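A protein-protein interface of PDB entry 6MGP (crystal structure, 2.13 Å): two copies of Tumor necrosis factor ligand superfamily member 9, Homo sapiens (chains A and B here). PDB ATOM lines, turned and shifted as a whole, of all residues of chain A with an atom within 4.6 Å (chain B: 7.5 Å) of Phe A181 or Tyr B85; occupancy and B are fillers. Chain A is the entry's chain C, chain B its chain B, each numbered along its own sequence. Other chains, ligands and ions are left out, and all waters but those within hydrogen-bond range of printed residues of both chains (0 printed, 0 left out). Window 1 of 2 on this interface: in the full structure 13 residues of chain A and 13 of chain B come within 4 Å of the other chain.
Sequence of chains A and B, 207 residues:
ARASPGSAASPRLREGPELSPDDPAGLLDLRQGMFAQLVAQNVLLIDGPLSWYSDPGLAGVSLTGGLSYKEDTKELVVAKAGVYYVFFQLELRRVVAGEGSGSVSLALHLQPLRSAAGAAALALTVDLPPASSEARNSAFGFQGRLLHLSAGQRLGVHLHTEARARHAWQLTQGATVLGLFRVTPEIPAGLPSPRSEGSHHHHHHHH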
ATOM      1  N   MET A  34     -16.855  -7.364  15.768  1.00  0.00           N
ATOM      2  CA  MET A  34     -17.201  -8.403  16.732  1.00  0.00           C
ATOM      3  C   MET A  34     -16.970  -9.772  16.099  1.00  0.00           C
ATOM      4  O   MET A  34     -17.668 -10.162  15.158  1.00  0.00           O
ATOM      5  CB  MET A  34     -18.645  -8.242  17.202  1.00  0.00           C
ATOM      6  N   PHE A  35     -15.989 -10.502  16.613  1.00  0.00           N
ATOM      7  CA  PHE A  35     -15.731 -11.852  16.141  1.00  0.00           C
ATOM      8  C   PHE A  35     -14.974 -12.598  17.225  1.00  0.00           C
ATOM      9  O   PHE A  35     -14.365 -11.993  18.113  1.00  0.00           O
ATOM     10  CB  PHE A  35     -14.946 -11.860  14.826  1.00  0.00           C
ATOM     11  CG  PHE A  35     -13.555 -11.312  14.942  1.00  0.00           C
ATOM     12  CD1 PHE A  35     -12.511 -12.114  15.370  1.00  0.00           C
ATOM     13  CD2 PHE A  35     -13.291  -9.996  14.610  1.00  0.00           C
ATOM     14  CE1 PHE A  35     -11.236 -11.613  15.479  1.00  0.00           C
ATOM     15  CE2 PHE A  35     -12.014  -9.492  14.709  1.00  0.00           C
ATOM     16  CZ  PHE A  35     -10.987 -10.301  15.150  1.00  0.00           C
ATOM     17  N   VAL A  83     -26.633 -10.329  13.697  1.00  0.00           N
ATOM     18  CA  VAL A  83     -26.645 -11.639  13.062  1.00  0.00           C
ATOM     19  C   VAL A  83     -25.198 -12.055  12.828  1.00  0.00           C
ATOM     20  O   VAL A  83     -24.399 -11.288  12.280  1.00  0.00           O
ATOM     21  CB  VAL A  83     -27.452 -11.633  11.755  1.00  0.00           C
ATOM     22  CG1 VAL A  83     -26.992 -12.753  10.831  1.00  0.00           C
ATOM     23  CG2 VAL A  83     -28.934 -11.758  12.056  1.00  0.00           C
ATOM     24  N   TYR A  84     -24.850 -13.252  13.278  1.00  0.00           N
ATOM     25  CA  TYR A  84     -23.504 -13.763  13.137  1.00  0.00           C
ATOM     26  C   TYR A  84     -23.499 -14.979  12.223  1.00  0.00           C
ATOM     27  O   TYR A  84     -24.454 -15.763  12.189  1.00  0.00           O
ATOM     28  CB  TYR A  84     -22.911 -14.147  14.495  1.00  0.00           C
ATOM     29  CG  TYR A  84     -22.673 -12.968  15.416  1.00  0.00           C
ATOM     30  CD1 TYR A  84     -23.738 -12.246  15.947  1.00  0.00           C
ATOM     31  CD2 TYR A  84     -21.384 -12.591  15.766  1.00  0.00           C
ATOM     32  CE1 TYR A  84     -23.519 -11.161  16.798  1.00  0.00           C
ATOM     33  CE2 TYR A  84     -21.154 -11.518  16.612  1.00  0.00           C
ATOM     34  CZ  TYR A  84     -22.222 -10.807  17.127  1.00  0.00           C
ATOM     35  OH  TYR A  84     -21.977  -9.745  17.969  1.00  0.00           O
ATOM     36  N   TYR A  85     -22.415 -15.118  11.466  1.00  0.00           N
ATOM     37  CA  TYR A  85     -22.085 -16.377  10.813  1.00  0.00           C
ATOM     38  C   TYR A  85     -21.318 -17.216  11.824  1.00  0.00           C
ATOM     39  O   TYR A  85     -20.174 -16.897  12.167  1.00  0.00           O
ATOM     40  CB  TYR A  85     -21.269 -16.139   9.546  1.00  0.00           C
ATOM     41  CG  TYR A  85     -20.865 -17.411   8.812  1.00  0.00           C
ATOM     42  CD1 TYR A  85     -21.778 -18.110   8.031  1.00  0.00           C
ATOM     43  CD2 TYR A  85     -19.567 -17.900   8.892  1.00  0.00           C
ATOM     44  CE1 TYR A  85     -21.408 -19.267   7.356  1.00  0.00           C
ATOM     45  CE2 TYR A  85     -19.188 -19.048   8.216  1.00  0.00           C
ATOM     46  CZ  TYR A  85     -20.112 -19.728   7.452  1.00  0.00           C
ATOM     47  OH  TYR A  85     -19.730 -20.865   6.780  1.00  0.00           O
ATOM     48  N   PHE A  87     -19.821 -20.941  13.042  1.00  0.00           N
ATOM     49  CA  PHE A  87     -19.332 -22.182  12.457  1.00  0.00           C
ATOM     50  C   PHE A  87     -18.534 -22.947  13.501  1.00  0.00           C
ATOM     51  O   PHE A  87     -17.894 -22.353  14.369  1.00  0.00           O
ATOM     52  CB  PHE A  87     -18.472 -21.921  11.206  1.00  0.00           C
ATOM     53  CG  PHE A  87     -17.200 -21.164  11.477  1.00  0.00           C
ATOM     54  CD1 PHE A  87     -16.027 -21.837  11.809  1.00  0.00           C
ATOM     55  CD2 PHE A  87     -17.168 -19.775  11.375  1.00  0.00           C
ATOM     56  CE1 PHE A  87     -14.855 -21.139  12.056  1.00  0.00           C
ATOM     57  CE2 PHE A  87     -15.996 -19.070  11.615  1.00  0.00           C
ATOM     58  CZ  PHE A  87     -14.840 -19.750  11.955  1.00  0.00           C
ATOM     59  N   PHE A 142     -17.239 -29.951   8.963  1.00  0.00           N
ATOM     60  CA  PHE A 142     -17.404 -28.510   9.106  1.00  0.00           C
ATOM     61  C   PHE A 142     -18.862 -28.150   8.857  1.00  0.00           C
ATOM     62  O   PHE A 142     -19.488 -28.702   7.948  1.00  0.00           O
ATOM     63  CB  PHE A 142     -16.491 -27.741   8.126  1.00  0.00           C
ATOM     64  CG  PHE A 142     -16.642 -26.240   8.198  1.00  0.00           C
ATOM     65  CD1 PHE A 142     -17.657 -25.590   7.504  1.00  0.00           C
ATOM     66  CD2 PHE A 142     -15.764 -25.478   8.956  1.00  0.00           C
ATOM     67  CE1 PHE A 142     -17.801 -24.217   7.582  1.00  0.00           C
ATOM     68  CE2 PHE A 142     -15.901 -24.104   9.028  1.00  0.00           C
ATOM     69  CZ  PHE A 142     -16.921 -23.474   8.339  1.00  0.00           C
ATOM     70  N   LEU A 180     -17.121 -17.354  15.052  1.00  0.00           N
ATOM     71  CA  LEU A 180     -18.271 -16.538  14.686  1.00  0.00           C
ATOM     72  C   LEU A 180     -17.806 -15.115  14.432  1.00  0.00           C
ATOM     73  O   LEU A 180     -16.906 -14.617  15.111  1.00  0.00           O
ATOM     74  CB  LEU A 180     -19.366 -16.555  15.771  1.00  0.00           C
ATOM     75  CG  LEU A 180     -19.167 -15.720  17.040  1.00  0.00           C
ATOM     76  CD1 LEU A 180     -20.458 -15.588  17.832  1.00  0.00           C
ATOM     77  CD2 LEU A 180     -18.105 -16.351  17.895  1.00  0.00           C
ATOM     78  N   PHE A 181     -18.413 -14.482  13.437  1.00  0.00           N
ATOM     79  CA  PHE A 181     -18.227 -13.062  13.203  1.00  0.00           C
ATOM     80  C   PHE A 181     -19.575 -12.457  12.855  1.00  0.00           C
ATOM     81  O   PHE A 181     -20.444 -13.128  12.290  1.00  0.00           O
ATOM     82  CB  PHE A 181     -17.204 -12.799  12.093  1.00  0.00           C
ATOM     83  CG  PHE A 181     -17.440 -13.599  10.841  1.00  0.00           C
ATOM     84  CD1 PHE A 181     -18.237 -13.097   9.825  1.00  0.00           C
ATOM     85  CD2 PHE A 181     -16.858 -14.845  10.675  1.00  0.00           C
ATOM     86  CE1 PHE A 181     -18.455 -13.821   8.666  1.00  0.00           C
ATOM     87  CE2 PHE A 181     -17.071 -15.577   9.517  1.00  0.00           C
ATOM     88  CZ  PHE A 181     -17.867 -15.065   8.511  1.00  0.00           C
ATOM     89  N   ARG A 182     -19.748 -11.184  13.210  1.00  0.00           N
ATOM     90  CA  ARG A 182     -20.994 -10.478  12.946  1.00  0.00           C
ATOM     91  C   ARG A 182     -21.038 -10.020  11.495  1.00  0.00           C
ATOM     92  O   ARG A 182     -20.081  -9.421  10.994  1.00  0.00           O
ATOM     93  CB  ARG A 182     -21.134  -9.275  13.877  1.00  0.00           C
ATOM     94  CG  ARG A 182     -22.385  -8.440  13.617  1.00  0.00           C
ATOM     95  CD  ARG A 182     -22.576  -7.373  14.673  1.00  0.00           C
ATOM     96  NE  ARG A 182     -21.542  -6.345  14.597  1.00  0.00           N
ATOM     97  CZ  ARG A 182     -21.581  -5.205  15.278  1.00  0.00           C
ATOM     98  NH1 ARG A 182     -22.610  -4.949  16.080  1.00  0.00           N
ATOM     99  NH2 ARG A 182     -20.598  -4.322  15.155  1.00  0.00           N
ATOM    100  N   VAL A 183     -22.157 -10.289  10.824  1.00  0.00           N
ATOM    101  CA  VAL A 183     -22.318  -9.874   9.434  1.00  0.00           C
ATOM    102  C   VAL A 183     -23.098  -8.571   9.287  1.00  0.00           C
ATOM    103  O   VAL A 183     -23.020  -7.942   8.221  1.00  0.00           O
ATOM    104  CB  VAL A 183     -22.990 -10.981   8.596  1.00  0.00           C
ATOM    105  CG1 VAL A 183     -22.200 -12.302   8.691  1.00  0.00           C
ATOM    106  CG2 VAL A 183     -24.431 -11.156   9.022  1.00  0.00           C
ATOM    107  N   ALA B  36     -11.044 -11.932  -1.809  1.00  0.00           N
ATOM    108  CA  ALA B  36     -10.481 -12.583  -2.981  1.00  0.00           C
ATOM    109  C   ALA B  36     -11.005 -14.010  -3.049  1.00  0.00           C
ATOM    110  O   ALA B  36     -11.252 -14.648  -2.021  1.00  0.00           O
ATOM    111  CB  ALA B  36      -8.945 -12.587  -2.960  1.00  0.00           C
ATOM    112  N   GLY B  82      -5.123  -7.871   9.201  1.00  0.00           N
ATOM    113  CA  GLY B  82      -6.458  -7.997   9.747  1.00  0.00           C
ATOM    114  C   GLY B  82      -6.815  -9.452   9.965  1.00  0.00           C
ATOM    115  O   GLY B  82      -6.024 -10.358   9.705  1.00  0.00           O
ATOM    116  N   VAL B  83      -8.034  -9.657  10.456  1.00  0.00           N
ATOM    117  CA  VAL B  83      -8.586 -10.995  10.624  1.00  0.00           C
ATOM    118  C   VAL B  83      -9.490 -11.292   9.440  1.00  0.00           C
ATOM    119  O   VAL B  83     -10.346 -10.476   9.078  1.00  0.00           O
ATOM    120  CB  VAL B  83      -9.342 -11.135  11.953  1.00  0.00           C
ATOM    121  CG1 VAL B  83     -10.003 -12.513  12.039  1.00  0.00           C
ATOM    122  CG2 VAL B  83      -8.374 -10.943  13.107  1.00  0.00           C
ATOM    123  N   TYR B  84      -9.286 -12.451   8.825  1.00  0.00           N
ATOM    124  CA  TYR B  84     -10.005 -12.868   7.633  1.00  0.00           C
ATOM    125  C   TYR B  84     -10.668 -14.209   7.881  1.00  0.00           C
ATOM    126  O   TYR B  84     -10.088 -15.091   8.519  1.00  0.00           O
ATOM    127  CB  TYR B  84      -9.066 -13.002   6.435  1.00  0.00           C
ATOM    128  CG  TYR B  84      -8.461 -11.713   5.938  1.00  0.00           C
ATOM    129  CD1 TYR B  84      -7.491 -11.048   6.674  1.00  0.00           C
ATOM    130  CD2 TYR B  84      -8.845 -11.170   4.719  1.00  0.00           C
ATOM    131  CE1 TYR B  84      -6.927  -9.865   6.212  1.00  0.00           C
ATOM    132  CE2 TYR B  84      -8.288  -9.990   4.251  1.00  0.00           C
ATOM    133  CZ  TYR B  84      -7.329  -9.344   4.999  1.00  0.00           C
ATOM    134  OH  TYR B  84      -6.775  -8.173   4.533  1.00  0.00           O
ATOM    135  N   TYR B  85     -11.890 -14.357   7.388  1.00  0.00           N
ATOM    136  CA  TYR B  85     -12.486 -15.677   7.242  1.00  0.00           C
ATOM    137  C   TYR B  85     -11.931 -16.279   5.963  1.00  0.00           C
ATOM    138  O   TYR B  85     -12.155 -15.738   4.876  1.00  0.00           O
ATOM    139  CB  TYR B  85     -14.009 -15.596   7.207  1.00  0.00           C
ATOM    140  CG  TYR B  85     -14.681 -16.945   6.992  1.00  0.00           C
ATOM    141  CD1 TYR B  85     -14.719 -17.899   8.009  1.00  0.00           C
ATOM    142  CD2 TYR B  85     -15.270 -17.266   5.772  1.00  0.00           C
ATOM    143  CE1 TYR B  85     -15.324 -19.137   7.813  1.00  0.00           C
ATOM    144  CE2 TYR B  85     -15.875 -18.496   5.568  1.00  0.00           C
ATOM    145  CZ  TYR B  85     -15.898 -19.433   6.592  1.00  0.00           C
ATOM    146  OH  TYR B  85     -16.509 -20.658   6.394  1.00  0.00           O
ATOM    147  N   VAL B  86     -11.166 -17.362   6.104  1.00  0.00           N
ATOM    148  CA  VAL B  86     -10.446 -17.997   5.005  1.00  0.00           C
ATOM    149  C   VAL B  86     -10.984 -19.408   4.827  1.00  0.00           C
ATOM    150  O   VAL B  86     -11.109 -20.159   5.801  1.00  0.00           O
ATOM    151  CB  VAL B  86      -8.930 -18.033   5.265  1.00  0.00           C
ATOM    152  CG1 VAL B  86      -8.206 -18.669   4.091  1.00  0.00           C
ATOM    153  CG2 VAL B  86      -8.403 -16.630   5.528  1.00  0.00           C
ATOM    154  N   PHE B  87     -11.291 -19.774   3.584  1.00  0.00           N
ATOM    155  CA  PHE B  87     -11.860 -21.079   3.290  1.00  0.00           C
ATOM    156  C   PHE B  87     -11.265 -21.612   1.996  1.00  0.00           C
ATOM    157  O   PHE B  87     -10.817 -20.845   1.140  1.00  0.00           O
ATOM    158  CB  PHE B  87     -13.391 -21.019   3.178  1.00  0.00           C
ATOM    159  CG  PHE B  87     -13.889 -20.106   2.082  1.00  0.00           C
ATOM    160  CD1 PHE B  87     -14.028 -18.744   2.303  1.00  0.00           C
ATOM    161  CD2 PHE B  87     -14.213 -20.611   0.829  1.00  0.00           C
ATOM    162  CE1 PHE B  87     -14.489 -17.896   1.294  1.00  0.00           C
ATOM    163  CE2 PHE B  87     -14.668 -19.775  -0.188  1.00  0.00           C
ATOM    164  CZ  PHE B  87     -14.808 -18.410   0.049  1.00  0.00           C
ATOM    165  N   PHE B  88     -11.220 -22.939   1.879  1.00  0.00           N
ATOM    166  CA  PHE B  88     -10.976 -23.554   0.585  1.00  0.00           C
ATOM    167  C   PHE B  88     -11.778 -24.844   0.488  1.00  0.00           C
ATOM    168  O   PHE B  88     -12.249 -25.394   1.487  1.00  0.00           O
ATOM    169  CB  PHE B  88      -9.465 -23.764   0.273  1.00  0.00           C
ATOM    170  CG  PHE B  88      -8.688 -24.627   1.260  1.00  0.00           C
ATOM    171  CD1 PHE B  88      -9.299 -25.337   2.281  1.00  0.00           C
ATOM    172  CD2 PHE B  88      -7.307 -24.720   1.134  1.00  0.00           C
ATOM    173  CE1 PHE B  88      -8.552 -26.120   3.158  1.00  0.00           C
ATOM    174  CE2 PHE B  88      -6.550 -25.502   2.006  1.00  0.00           C
ATOM    175  CZ  PHE B  88      -7.176 -26.206   3.016  1.00  0.00           C
ATOM    176  N   LEU B 122      -4.723 -24.072   7.374  1.00  0.00           N
ATOM    177  CA  LEU B 122      -5.929 -24.699   6.868  1.00  0.00           C
ATOM    178  C   LEU B 122      -5.506 -26.023   6.257  1.00  0.00           C
ATOM    179  O   LEU B 122      -4.588 -26.060   5.431  1.00  0.00           O
ATOM    180  CB  LEU B 122      -6.611 -23.812   5.819  1.00  0.00           C
ATOM    181  CG  LEU B 122      -8.113 -23.539   5.856  1.00  0.00           C
ATOM    182  CD1 LEU B 122      -8.554 -23.204   7.255  1.00  0.00           C
ATOM    183  CD2 LEU B 122      -8.462 -22.399   4.900  1.00  0.00           C
ATOM    184  N   PHE B 142     -14.595 -29.298   2.404  1.00  0.00           N
ATOM    185  CA  PHE B 142     -14.618 -27.852   2.608  1.00  0.00           C
ATOM    186  C   PHE B 142     -14.127 -27.546   4.018  1.00  0.00           C
ATOM    187  O   PHE B 142     -14.576 -28.184   4.974  1.00  0.00           O
ATOM    188  CB  PHE B 142     -16.040 -27.289   2.411  1.00  0.00           C
ATOM    189  CG  PHE B 142     -16.181 -25.831   2.765  1.00  0.00           C
ATOM    190  CD1 PHE B 142     -16.431 -25.438   4.070  1.00  0.00           C
ATOM    191  CD2 PHE B 142     -16.076 -24.851   1.783  1.00  0.00           C
ATOM    192  CE1 PHE B 142     -16.551 -24.092   4.391  1.00  0.00           C
ATOM    193  CE2 PHE B 142     -16.200 -23.513   2.099  1.00  0.00           C
ATOM    194  CZ  PHE B 142     -16.435 -23.136   3.404  1.00  0.00           C
ATOM    195  N   GLN B 143     -13.243 -26.549   4.154  1.00  0.00           N
ATOM    196  CA  GLN B 143     -12.874 -26.037   5.471  1.00  0.00           C
ATOM    197  C   GLN B 143     -12.769 -24.511   5.468  1.00  0.00           C
ATOM    198  O   GLN B 143     -12.345 -23.906   4.480  1.00  0.00           O
ATOM    199  CB  GLN B 143     -11.547 -26.634   5.961  1.00  0.00           C
ATOM    200  CG  GLN B 143     -11.218 -26.285   7.409  1.00  0.00           C
ATOM    201  CD  GLN B 143      -9.840 -26.756   7.826  1.00  0.00           C
ATOM    202  OE1 GLN B 143      -8.828 -26.359   7.242  1.00  0.00           O
ATOM    203  NE2 GLN B 143      -9.790 -27.607   8.845  1.00  0.00           N
ATOM    204  N   GLY B 144     -13.152 -23.895   6.584  1.00  0.00           N
ATOM    205  CA  GLY B 144     -12.933 -22.476   6.782  1.00  0.00           C
ATOM    206  C   GLY B 144     -12.610 -22.200   8.236  1.00  0.00           C
ATOM    207  O   GLY B 144     -12.951 -22.983   9.128  1.00  0.00           O
ATOM    208  N   ARG B 145     -11.927 -21.080   8.464  1.00  0.00           N
ATOM    209  CA  ARG B 145     -11.719 -20.572   9.816  1.00  0.00           C
ATOM    210  C   ARG B 145     -11.244 -19.127   9.731  1.00  0.00           C
ATOM    211  O   ARG B 145     -10.953 -18.606   8.650  1.00  0.00           O
ATOM    212  CB  ARG B 145     -10.727 -21.431  10.607  1.00  0.00           C
ATOM    213  CG  ARG B 145      -9.274 -21.175  10.292  1.00  0.00           C
ATOM    214  CD  ARG B 145      -8.432 -22.381  10.678  1.00  0.00           C
ATOM    215  NE  ARG B 145      -7.982 -22.346  12.066  1.00  0.00           N
ATOM    216  CZ  ARG B 145      -7.859 -23.426  12.831  1.00  0.00           C
ATOM    217  NH1 ARG B 145      -8.163 -24.622  12.340  1.00  0.00           N
ATOM    218  NH2 ARG B 145      -7.436 -23.311  14.085  1.00  0.00           N
ATOM    219  N   LEU B 146     -11.171 -18.485  10.893  1.00  0.00           N
ATOM    220  CA  LEU B 146     -10.632 -17.135  11.001  1.00  0.00           C
ATOM    221  C   LEU B 146      -9.120 -17.188  11.201  1.00  0.00           C
ATOM    222  O   LEU B 146      -8.630 -17.871  12.109  1.00  0.00           O
ATOM    223  CB  LEU B 146     -11.295 -16.384  12.156  1.00  0.00           C
ATOM    224  CG  LEU B 146     -12.812 -16.224  12.047  1.00  0.00           C
ATOM    225  CD1 LEU B 146     -13.411 -15.685  13.337  1.00  0.00           C
ATOM    226  CD2 LEU B 146     -13.169 -15.329  10.870  1.00  0.00           C
ATOM    227  N   LEU B 147      -8.387 -16.479  10.346  1.00  0.00           N
ATOM    228  CA  LEU B 147      -6.947 -16.334  10.486  1.00  0.00           C
ATOM    229  C   LEU B 147      -6.572 -14.859  10.578  1.00  0.00           C
ATOM    230  O   LEU B 147      -7.123 -14.015   9.861  1.00  0.00           O
ATOM    231  CB  LEU B 147      -6.199 -16.984   9.317  1.00  0.00           C
ATOM    232  CG  LEU B 147      -6.549 -18.438   9.002  1.00  0.00           C
ATOM    233  CD1 LEU B 147      -5.893 -18.828   7.701  1.00  0.00           C
ATOM    234  CD2 LEU B 147      -6.116 -19.369  10.136  1.00  0.00           C
ATOM    235  N   HIS B 148      -5.643 -14.550  11.476  1.00  0.00           N
ATOM    236  CA  HIS B 148      -5.026 -13.229  11.500  1.00  0.00           C
ATOM    237  C   HIS B 148      -3.903 -13.211  10.471  1.00  0.00           C
ATOM    238  O   HIS B 148      -2.906 -13.930  10.615  1.00  0.00           O
ATOM    239  CB  HIS B 148      -4.503 -12.891  12.891  1.00  0.00           C
ATOM    240  CG  HIS B 148      -3.765 -11.588  12.948  1.00  0.00           C
ATOM    241  ND1 HIS B 148      -4.393 -10.387  13.212  1.00  0.00           N
ATOM    242  CD2 HIS B 148      -2.458 -11.293  12.750  1.00  0.00           C
ATOM    243  CE1 HIS B 148      -3.502  -9.413  13.185  1.00  0.00           C
ATOM    244  NE2 HIS B 148      -2.321  -9.934  12.907  1.00  0.00           N
ATOM    245  N   LEU B 149      -4.062 -12.404   9.426  1.00  0.00           N
ATOM    246  CA  LEU B 149      -3.074 -12.284   8.364  1.00  0.00           C
ATOM    247  C   LEU B 149      -2.354 -10.946   8.496  1.00  0.00           C
ATOM    248  O   LEU B 149      -3.000  -9.898   8.613  1.00  0.00           O
ATOM    249  CB  LEU B 149      -3.738 -12.411   6.988  1.00  0.00           C
ATOM    250  CG  LEU B 149      -4.540 -13.685   6.703  1.00  0.00           C
ATOM    251  CD1 LEU B 149      -5.087 -13.649   5.293  1.00  0.00           C
ATOM    252  CD2 LEU B 149      -3.694 -14.936   6.911  1.00  0.00           C
ATOM    253  N   GLY B 179     -10.780 -18.952  -1.004  1.00  0.00           N
ATOM    254  CA  GLY B 179     -11.455 -17.683  -0.820  1.00  0.00           C
ATOM    255  C   GLY B 179     -11.185 -17.106   0.555  1.00  0.00           C
ATOM    256  O   GLY B 179     -10.817 -17.817   1.495  1.00  0.00           O
ATOM    257  N   LEU B 180     -11.374 -15.793   0.655  1.00  0.00           N
ATOM    258  CA  LEU B 180     -11.252 -15.111   1.936  1.00  0.00           C
ATOM    259  C   LEU B 180     -11.818 -13.704   1.820  1.00  0.00           C
ATOM    260  O   LEU B 180     -11.784 -13.087   0.750  1.00  0.00           O
ATOM    261  CB  LEU B 180      -9.796 -15.067   2.419  1.00  0.00           C
ATOM    262  CG  LEU B 180      -8.881 -13.924   1.990  1.00  0.00           C
ATOM    263  CD1 LEU B 180      -7.605 -13.986   2.786  1.00  0.00           C
ATOM    264  CD2 LEU B 180      -8.567 -14.006   0.515  1.00  0.00           C
ATOM    265  N   PHE B 181     -12.369 -13.221   2.928  1.00  0.00           N
ATOM    266  CA  PHE B 181     -12.792 -11.837   3.043  1.00  0.00           C
ATOM    267  C   PHE B 181     -12.491 -11.362   4.452  1.00  0.00           C
ATOM    268  O   PHE B 181     -12.553 -12.136   5.413  1.00  0.00           O
ATOM    269  CB  PHE B 181     -14.284 -11.652   2.720  1.00  0.00           C
ATOM    270  CG  PHE B 181     -15.192 -12.594   3.459  1.00  0.00           C
ATOM    271  CD1 PHE B 181     -15.641 -12.289   4.734  1.00  0.00           C
ATOM    272  CD2 PHE B 181     -15.608 -13.779   2.874  1.00  0.00           C
ATOM    273  CE1 PHE B 181     -16.488 -13.142   5.417  1.00  0.00           C
ATOM    274  CE2 PHE B 181     -16.455 -14.645   3.552  1.00  0.00           C
ATOM    275  CZ  PHE B 181     -16.897 -14.321   4.828  1.00  0.00           C
ATOM    276  N   ARG B 182     -12.157 -10.081   4.567  1.00  0.00           N
ATOM    277  CA  ARG B 182     -11.778  -9.517   5.850  1.00  0.00           C
ATOM    278  C   ARG B 182     -13.014  -9.283   6.703  1.00  0.00           C
ATOM    279  O   ARG B 182     -14.001  -8.708   6.237  1.00  0.00           O
ATOM    280  CB  ARG B 182     -11.014  -8.208   5.656  1.00  0.00           C
ATOM    281  CG  ARG B 182     -10.296  -7.748   6.911  1.00  0.00           C
ATOM    282  CD  ARG B 182      -9.416  -6.548   6.647  1.00  0.00           C
ATOM    283  NE  ARG B 182     -10.146  -5.477   5.977  1.00  0.00           N
ATOM    284  CZ  ARG B 182      -9.749  -4.211   5.967  1.00  0.00           C
ATOM    285  NH1 ARG B 182      -8.633  -3.871   6.598  1.00  0.00           N
ATOM    286  NH2 ARG B 182     -10.463  -3.288   5.331  1.00  0.00           N
ATOM    287  N   VAL B 183     -12.968  -9.748   7.947  1.00  0.00           N
ATOM    288  CA  VAL B 183     -14.025  -9.410   8.889  1.00  0.00           C
ATOM    289  C   VAL B 183     -13.686  -8.119   9.624  1.00  0.00           C
ATOM    290  O   VAL B 183     -14.597  -7.379  10.011  1.00  0.00           O
ATOM    291  CB  VAL B 183     -14.287 -10.572   9.862  1.00  0.00           C
ATOM    292  CG1 VAL B 183     -14.667 -11.821   9.084  1.00  0.00           C
ATOM    293  CG2 VAL B 183     -13.068 -10.855  10.707  1.00  0.00           C
ATOM    294  N   THR B 184     -12.394  -7.838   9.815  1.00  0.00           N
ATOM    295  CA  THR B 184     -11.877  -6.480  10.023  1.00  0.00           C
ATOM    296  C   THR B 184     -10.354  -6.464  10.154  1.00  0.00           C
ATOM    297  O   THR B 184      -9.760  -7.307  10.826  1.00  0.00           O
ATOM    298  CB  THR B 184     -12.474  -5.794  11.256  1.00  0.00           C
ATOM    299  OG1 THR B 184     -12.031  -4.429  11.291  1.00  0.00           O
ATOM    300  CG2 THR B 184     -12.077  -6.515  12.540  1.00  0.00           C
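Tyr B85 touches its own counterpart, Tyr A85. Phe A87 touches Tyr B85, but with the chains exchanged Tyr A85 does not touch Phe B87 (7.3 Å). Phe A142 touches Tyr B85, but with the chains exchanged Tyr A85 does not touch Phe B142 (5.1 Å). Phe A181 touches Tyr B85, but with the chains exchanged Tyr A85 does not touch Phe B181 (6.0 Å). 9 positions are printed for both chains.
Hydrophobic or aromatic side chains of chain B that line the printed part of chain A: Val B83, Tyr B85, Phe B142, Leu B146, Phe B181 and Val B183. Among the printed residues, no Asp or Glu carboxylate lies within 4 Å of a Lys or Arg side-chain nitrogen of the other chain.
OH of Tyr B85 lies within hydrogen-bond range of OH of Tyr A85 (3.3 Å).
The backbone NH (N) of Val B86 sits at hydrogen-bond distance from the backbone carbonyl oxygen (O) of Arg B145. The backbone NH (N) of Val B83 sits at hydrogen-bond distance from the backbone carbonyl oxygen (O) of Thr B184 (2.9 Å). O of Val B83 sits at hydrogen-bond distance from N of Val B183 (2.9 Å). The backbone carbonyl oxygen (O) of Phe A181 is in hydrogen-bond range of the backbone NH (N) of Tyr A85. N of Tyr B85 sits at hydrogen-bond distance from O of Phe B181 (3.0 Å).
Among the printed residues, merely in contact across the chains: Phe A142 with Gly B144 (3.2 Å), Phe A35 with Val B83 (3.4 Å), Phe A142 with Phe B142 (3.4 Å), Phe A142 with Tyr B85 (3.4 Å), Phe A181 with Tyr B85 (3.6 Å), Phe A35 with Thr B184 (3.7 Å), Phe A181 with Leu B146 (3.7 Å), Phe A181 with Val B183 (3.7 Å), Phe A181 with Phe B181 (3.9 Å), Phe A87 with Tyr B85 (3.9 Å), Phe A87 with Arg B145 (3.9 Å) and Phe A87 with Gly B144 (3.9 Å).
Printed residues of chain B within 4 Å of Tyr A85: Tyr B85. Of the printed residues of chain B, Phe A87 touches Tyr B85 (3.9 Å), Gly B144 (3.9 Å) and Arg B145 (3.9 Å). Of the printed residues of chain B, Phe A142 touches Tyr B85 (3.4 Å), Phe B142 (3.4 Å) and Gly B144 (3.2 Å). Phe A181 touches just these residues of chain B: Tyr B85, Leu B146, Phe B181 and Val B183. Val B86 touches none of the printed residues of chain A. Of the printed residues of chain A, Gly B144 touches Phe A87 and Phe A142. Of the printed residues of chain A, Val B183 touches Phe A181 (3.7 Å). The nearest printed residue of chain A that does not touch Val B183 is Phe A35 (4.003 Å).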
